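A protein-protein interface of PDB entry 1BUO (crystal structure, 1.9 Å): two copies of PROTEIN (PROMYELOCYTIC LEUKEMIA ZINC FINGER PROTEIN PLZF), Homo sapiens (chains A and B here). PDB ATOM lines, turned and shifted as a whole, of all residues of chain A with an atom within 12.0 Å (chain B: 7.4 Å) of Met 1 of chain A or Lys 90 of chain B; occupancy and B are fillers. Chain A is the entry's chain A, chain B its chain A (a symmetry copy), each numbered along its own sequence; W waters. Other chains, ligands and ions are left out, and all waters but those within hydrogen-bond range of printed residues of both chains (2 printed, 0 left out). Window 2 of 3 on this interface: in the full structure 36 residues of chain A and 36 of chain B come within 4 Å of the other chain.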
ATOM      1  N   MET A   1      25.709   5.615 -37.426  1.00  0.00           N
ATOM      2  CA  MET A   1      26.186   4.258 -36.986  1.00  0.00           C
ATOM      3  C   MET A   1      25.045   3.329 -36.525  1.00  0.00           C
ATOM      4  O   MET A   1      23.878   3.742 -36.581  1.00  0.00           O
ATOM      5  CB  MET A   1      27.145   4.376 -35.813  1.00  0.00           C
ATOM      6  CG  MET A   1      28.590   3.970 -36.068  1.00  0.00           C
ATOM      7  SD  MET A   1      29.714   5.376 -36.064  1.00  0.00           S
ATOM      8  CE  MET A   1      28.984   6.379 -34.758  1.00  0.00           C
ATOM      9  N   GLY A   2      25.440   2.139 -36.062  1.00  0.00           N
ATOM     10  CA  GLY A   2      24.537   1.143 -35.512  1.00  0.00           C
ATOM     11  C   GLY A   2      24.664   1.245 -33.945  1.00  0.00           C
ATOM     12  O   GLY A   2      25.676   1.724 -33.423  1.00  0.00           O
ATOM     13  N   MET A   3      23.566   1.038 -33.224  1.00  0.00           N
ATOM     14  CA  MET A   3      23.632   1.191 -31.748  1.00  0.00           C
ATOM     15  C   MET A   3      22.815   0.019 -31.260  1.00  0.00           C
ATOM     16  O   MET A   3      21.952  -0.431 -32.003  1.00  0.00           O
ATOM     17  CB  MET A   3      23.116   2.530 -31.183  1.00  0.00           C
ATOM     18  CG  MET A   3      21.999   2.553 -30.140  1.00  0.00           C
ATOM     19  SD  MET A   3      21.618   4.181 -29.389  1.00  0.00           S
ATOM     20  CE  MET A   3      19.847   4.124 -29.746  1.00  0.00           C
ATOM     21  N   ILE A   4      23.096  -0.413 -30.005  1.00  0.00           N
ATOM     22  CA  ILE A   4      22.181  -1.382 -29.392  1.00  0.00           C
ATOM     23  C   ILE A   4      21.675  -0.626 -28.066  1.00  0.00           C
ATOM     24  O   ILE A   4      22.344   0.234 -27.641  1.00  0.00           O
ATOM     25  CB  ILE A   4      23.068  -2.553 -28.990  1.00  0.00           C
ATOM     26  CG1 ILE A   4      22.891  -3.654 -30.050  1.00  0.00           C
ATOM     27  CG2 ILE A   4      23.041  -3.070 -27.585  1.00  0.00           C
ATOM     28  CD1 ILE A   4      23.997  -3.409 -31.057  1.00  0.00           C
ATOM     29  N   GLN A   5      20.428  -0.865 -27.786  1.00  0.00           N
ATOM     30  CA  GLN A   5      19.769  -0.201 -26.662  1.00  0.00           C
ATOM     31  C   GLN A   5      19.051  -1.276 -25.867  1.00  0.00           C
ATOM     32  O   GLN A   5      18.386  -2.172 -26.345  1.00  0.00           O
ATOM     33  CB  GLN A   5      18.764   0.879 -27.109  1.00  0.00           C
ATOM     34  CG  GLN A   5      18.242   1.633 -25.844  1.00  0.00           C
ATOM     35  CD  GLN A   5      17.238   2.720 -26.285  1.00  0.00           C
ATOM     36  OE1 GLN A   5      17.799   3.739 -26.611  1.00  0.00           O
ATOM     37  NE2 GLN A   5      15.977   2.326 -26.270  1.00  0.00           N
ATOM     38  N   LEU A   6      19.232  -1.158 -24.498  1.00  0.00           N
ATOM     39  CA  LEU A   6      18.441  -2.122 -23.685  1.00  0.00           C
ATOM     40  C   LEU A   6      17.770  -1.207 -22.623  1.00  0.00           C
ATOM     41  O   LEU A   6      18.411  -0.283 -22.098  1.00  0.00           O
ATOM     42  CB  LEU A   6      19.466  -2.997 -22.961  1.00  0.00           C
ATOM     43  CG  LEU A   6      20.525  -3.807 -23.678  1.00  0.00           C
ATOM     44  CD1 LEU A   6      21.427  -4.560 -22.691  1.00  0.00           C
ATOM     45  CD2 LEU A   6      19.828  -4.792 -24.643  1.00  0.00           C
ATOM     46  N   LYS B  73      34.823   2.984 -20.478  1.00  0.00           N
ATOM     47  CA  LYS B  73      33.682   3.042 -21.362  1.00  0.00           C
ATOM     48  C   LYS B  73      32.547   2.120 -20.936  1.00  0.00           C
ATOM     49  O   LYS B  73      31.388   2.514 -21.059  1.00  0.00           O
ATOM     50  CB  LYS B  73      34.043   2.628 -22.812  1.00  0.00           C
ATOM     51  CG  LYS B  73      32.833   2.564 -23.720  1.00  0.00           C
ATOM     52  CD  LYS B  73      33.184   2.649 -25.199  1.00  0.00           C
ATOM     53  CE  LYS B  73      33.761   1.352 -25.707  1.00  0.00           C
ATOM     54  NZ  LYS B  73      33.192   0.923 -27.019  1.00  0.00           N
ATOM     55  N   GLN B  77      28.676   3.143 -19.384  1.00  0.00           N
ATOM     56  CA  GLN B  77      27.529   2.534 -19.939  1.00  0.00           C
ATOM     57  C   GLN B  77      26.614   1.972 -18.858  1.00  0.00           C
ATOM     58  O   GLN B  77      25.419   2.192 -18.815  1.00  0.00           O
ATOM     59  CB  GLN B  77      27.791   1.488 -20.996  1.00  0.00           C
ATOM     60  CG  GLN B  77      28.341   2.127 -22.294  1.00  0.00           C
ATOM     61  CD  GLN B  77      28.963   1.122 -23.210  1.00  0.00           C
ATOM     62  OE1 GLN B  77      29.278  -0.033 -22.863  1.00  0.00           O
ATOM     63  NE2 GLN B  77      29.138   1.451 -24.493  1.00  0.00           N
ATOM     64  N   LEU B  87      20.387   1.525 -21.443  1.00  0.00           N
ATOM     65  CA  LEU B  87      21.853   1.520 -21.733  1.00  0.00           C
ATOM     66  C   LEU B  87      22.000   1.544 -23.330  1.00  0.00           C
ATOM     67  O   LEU B  87      21.234   0.809 -23.903  1.00  0.00           O
ATOM     68  CB  LEU B  87      22.322   0.117 -21.338  1.00  0.00           C
ATOM     69  CG  LEU B  87      23.817  -0.192 -21.577  1.00  0.00           C
ATOM     70  CD1 LEU B  87      24.317  -1.044 -20.419  1.00  0.00           C
ATOM     71  CD2 LEU B  87      23.984  -0.926 -22.911  1.00  0.00           C
ATOM     72  N   GLN B  88      22.965   2.386 -23.681  1.00  0.00           N
ATOM     73  CA  GLN B  88      23.196   2.395 -25.127  1.00  0.00           C
ATOM     74  C   GLN B  88      24.644   1.966 -25.381  1.00  0.00           C
ATOM     75  O   GLN B  88      25.526   2.464 -24.669  1.00  0.00           O
ATOM     76  CB  GLN B  88      22.886   3.813 -25.685  1.00  0.00           C
ATOM     77  CG  GLN B  88      21.423   4.159 -25.358  1.00  0.00           C
ATOM     78  CD  GLN B  88      20.892   5.354 -26.137  1.00  0.00           C
ATOM     79  OE1 GLN B  88      21.693   6.285 -26.089  1.00  0.00           O
ATOM     80  NE2 GLN B  88      19.712   5.281 -26.763  1.00  0.00           N
ATOM     81  N   ALA B  89      24.807   1.118 -26.409  1.00  0.00           N
ATOM     82  CA  ALA B  89      26.186   0.707 -26.686  1.00  0.00           C
ATOM     83  C   ALA B  89      26.318   0.337 -28.184  1.00  0.00           C
ATOM     84  O   ALA B  89      25.333   0.406 -28.921  1.00  0.00           O
ATOM     85  CB  ALA B  89      26.542  -0.518 -25.808  1.00  0.00           C
ATOM     86  N   LYS B  90      27.534  -0.015 -28.547  1.00  0.00           N
ATOM     87  CA  LYS B  90      27.828  -0.534 -29.906  1.00  0.00           C
ATOM     88  C   LYS B  90      27.752  -2.043 -29.898  1.00  0.00           C
ATOM     89  O   LYS B  90      27.958  -2.671 -28.825  1.00  0.00           O
ATOM     90  CB  LYS B  90      29.199  -0.073 -30.421  1.00  0.00           C
ATOM     91  CG  LYS B  90      29.010   1.368 -30.901  1.00  0.00           C
ATOM     92  CD  LYS B  90      30.347   2.032 -31.183  1.00  0.00           C
ATOM     93  CE  LYS B  90      30.129   3.129 -32.237  1.00  0.00           C
ATOM     94  NZ  LYS B  90      29.571   2.519 -33.486  1.00  0.00           N
ATOM     95  N   ALA B  91      27.426  -2.721 -31.000  1.00  0.00           N
ATOM     96  CA  ALA B  91      27.350  -4.197 -30.957  1.00  0.00           C
ATOM     97  C   ALA B  91      28.626  -4.872 -30.494  1.00  0.00           C
ATOM     98  O   ALA B  91      28.626  -5.945 -29.836  1.00  0.00           O
ATOM     99  CB  ALA B  91      27.069  -4.787 -32.362  1.00  0.00           C
ATOM    100  N   GLU B  92      29.772  -4.296 -30.777  1.00  0.00           N
ATOM    101  CA  GLU B  92      31.074  -4.803 -30.358  1.00  0.00           C
ATOM    102  C   GLU B  92      31.328  -4.679 -28.830  1.00  0.00           C
ATOM    103  O   GLU B  92      32.436  -4.894 -28.313  1.00  0.00           O
ATOM    104  CB  GLU B  92      32.131  -3.907 -30.998  1.00  0.00           C
ATOM    105  CG  GLU B  92      32.211  -2.529 -30.398  1.00  0.00           C
ATOM    106  CD  GLU B  92      32.964  -1.485 -31.193  1.00  0.00           C
ATOM    107  OE1 GLU B  92      33.132  -1.711 -32.413  1.00  0.00           O
ATOM    108  OE2 GLU B  92      33.349  -0.445 -30.600  1.00  0.00           O
ATOM    109  N   ASP B  93      30.363  -4.073 -28.123  1.00  0.00           N
ATOM    110  CA  ASP B  93      30.567  -3.848 -26.674  1.00  0.00           C
ATOM    111  C   ASP B  93      29.804  -4.926 -25.951  1.00  0.00           C
ATOM    112  O   ASP B  93      29.903  -4.904 -24.678  1.00  0.00           O
ATOM    113  CB  ASP B  93      29.993  -2.497 -26.272  1.00  0.00           C
ATOM    114  CG  ASP B  93      30.578  -1.235 -26.777  1.00  0.00           C
ATOM    115  OD1 ASP B  93      31.773  -1.241 -27.139  1.00  0.00           O
ATOM    116  OD2 ASP B  93      29.935  -0.139 -26.823  1.00  0.00           O
ATOM    117  N   LEU B  94      28.996  -5.773 -26.533  1.00  0.00           N
ATOM    118  CA  LEU B  94      28.145  -6.727 -25.947  1.00  0.00           C
ATOM    119  C   LEU B  94      28.879  -7.771 -25.070  1.00  0.00           C
ATOM    120  O   LEU B  94      28.476  -7.931 -23.889  1.00  0.00           O
ATOM    121  CB  LEU B  94      27.198  -7.425 -26.888  1.00  0.00           C
ATOM    122  CG  LEU B  94      25.954  -6.631 -27.287  1.00  0.00           C
ATOM    123  CD1 LEU B  94      25.223  -7.350 -28.420  1.00  0.00           C
ATOM    124  CD2 LEU B  94      24.941  -6.412 -26.151  1.00  0.00           C
ATOM    125  N   ASP B  95      30.024  -8.224 -25.568  1.00  0.00           N
ATOM    126  CA  ASP B  95      30.797  -9.216 -24.760  1.00  0.00           C
ATOM    127  C   ASP B  95      31.375  -8.522 -23.534  1.00  0.00           C
ATOM    128  O   ASP B  95      31.349  -9.122 -22.441  1.00  0.00           O
ATOM    129  CB  ASP B  95      31.840  -9.786 -25.744  1.00  0.00           C
ATOM    130  CG  ASP B  95      32.791  -8.734 -26.246  1.00  0.00           C
ATOM    131  OD1 ASP B  95      32.607  -7.481 -26.223  1.00  0.00           O
ATOM    132  OD2 ASP B  95      33.905  -9.072 -26.719  1.00  0.00           O
ATOM    133  N   ASP B  96      31.881  -7.283 -23.623  1.00  0.00           N
ATOM    134  CA  ASP B  96      32.403  -6.513 -22.535  1.00  0.00           C
ATOM    135  C   ASP B  96      31.308  -6.231 -21.499  1.00  0.00           C
ATOM    136  O   ASP B  96      31.591  -6.257 -20.246  1.00  0.00           O
ATOM    137  CB  ASP B  96      33.057  -5.193 -22.865  1.00  0.00           C
ATOM    138  CG  ASP B  96      33.967  -5.223 -24.088  1.00  0.00           C
ATOM    139  OD1 ASP B  96      33.489  -5.445 -25.231  1.00  0.00           O
ATOM    140  OD2 ASP B  96      35.172  -5.035 -23.852  1.00  0.00           O
ATOM    141  N   LEU B  97      30.131  -5.915 -22.005  1.00  0.00           N
ATOM    142  CA  LEU B  97      29.008  -5.558 -21.106  1.00  0.00           C
ATOM    143  C   LEU B  97      28.504  -6.802 -20.379  1.00  0.00           C
ATOM    144  O   LEU B  97      28.265  -6.743 -19.169  1.00  0.00           O
ATOM    145  CB  LEU B  97      27.741  -4.993 -21.879  1.00  0.00           C
ATOM    146  CG  LEU B  97      28.033  -3.557 -22.222  1.00  0.00           C
ATOM    147  CD1 LEU B  97      27.054  -3.109 -23.361  1.00  0.00           C
ATOM    148  CD2 LEU B  97      27.889  -2.565 -21.054  1.00  0.00           C
HETATM  149  O   HOH W   1      28.455   1.123 -35.605  1.00  0.00           O
HETATM  150  O   HOH W   2      27.116  -1.132 -33.290  1.00  0.00           O
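SD of Met 3 of chain A sits close to NE2 of Gln 88 of chain B.
The backbone NH (N) of Ile 4 of chain A sits at hydrogen-bond distance from the backbone carbonyl oxygen (O) of Ala 89 of chain B.
The side-chain amide oxygen of Gln 5 of chain A sits at hydrogen-bond distance from the side-chain amide nitrogen of Gln 88 of chain B (2.5 Å).
The backbone carbonyl oxygen (O) of Leu 6 of chain A is in hydrogen-bond range of the backbone NH (N) of Leu 87 of chain B, at 2.8 Å.
The side-chain carboxylate (OD2) of Asp 93 of chain B lies within hydrogen-bond range of the backbone NH (N) of Lys 90 of chain B, 3.0 Å away.
Met 1 of chain A touches Lys 90 of chain B.
O of Gly 2 of chain A touches NZ of Lys 90 of chain B (3.98 Å).
Met 3 of chain A touches Ala 89 of chain B.
O of Ile 4 of chain A touches O of Leu 87 of chain B, 3.9 Å away.
CA of Gln 88 of chain B touches O of Ile 4 of chain A, 3.4 Å away.
Ile 4 of chain A touches Ala 91 of chain B.
CA of Gln 5 of chain A touches O of Leu 87 of chain B, 3.3 Å away.
Of chain B, only Lys 90 comes within 4 Å of Met 1 of chain A.
Of the printed residues of chain B, Gly 2 of chain A touches Lys 90 (3.98 Å).
Of the printed residues of chain B, Ile 4 of chain A touches Leu 87, Gln 88, Ala 89 and Ala 91.
Of the printed residues of chain B, Leu 6 of chain A touches Leu 87.
Of the printed residues of chain A, Lys 90 of chain B touches Met 1 (3.1 Å) and Gly 2 (3.98 Å).
No residue of chain A comes within 4 Å of Glu 92 of chain B.
No residue of chain A comes within 4 Å of Asp 93 of chain B.
No residue of chain A comes within 4 Å of Leu 94 of chain B.
The nearest printed residue of chain B that does not touch Met 1 of chain A is Glu 92 of chain B (8.1 Å).
The nearest printed residue of chain A that does not touch Gln 88 of chain B is Leu 6 of chain A (5.2 Å).
Of the 6 printed residues of chain A, 6 touch a printed residue of chain B.
Hydrophobic or aromatic side chains of chain A within 4 Å of the printed part of chain B: Met 1, Met 3 and Ile 4.
Of the 13 printed residues of chain B, 5 touch a printed residue of chain A.
Printed residues of chain B that touch a printed residue of chain A: Leu 87, Gln 88, Ala 89, Lys 90 and Ala 91.
Among the printed residues, no Asp or Glu carboxylate lies within 4 Å of a Lys or Arg side-chain nitrogen of the other chain.
No position is printed for both chains.
Of the 11 pairs that touch across the chains among the printed residues, none has its exchanged pair printed and touching as well.
Water W1 lies within hydrogen-bond range of the side-chain amino group (NZ) of Lys 90 of chain B (2.8 Å) and the backbone NH (N) of Gly 2 of chain A (3.2 Å).
Water W2 bridges the backbone NH (N) of Ala 91 of chain B and the backbone carbonyl oxygen (O) of Gly 2 of chain A.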
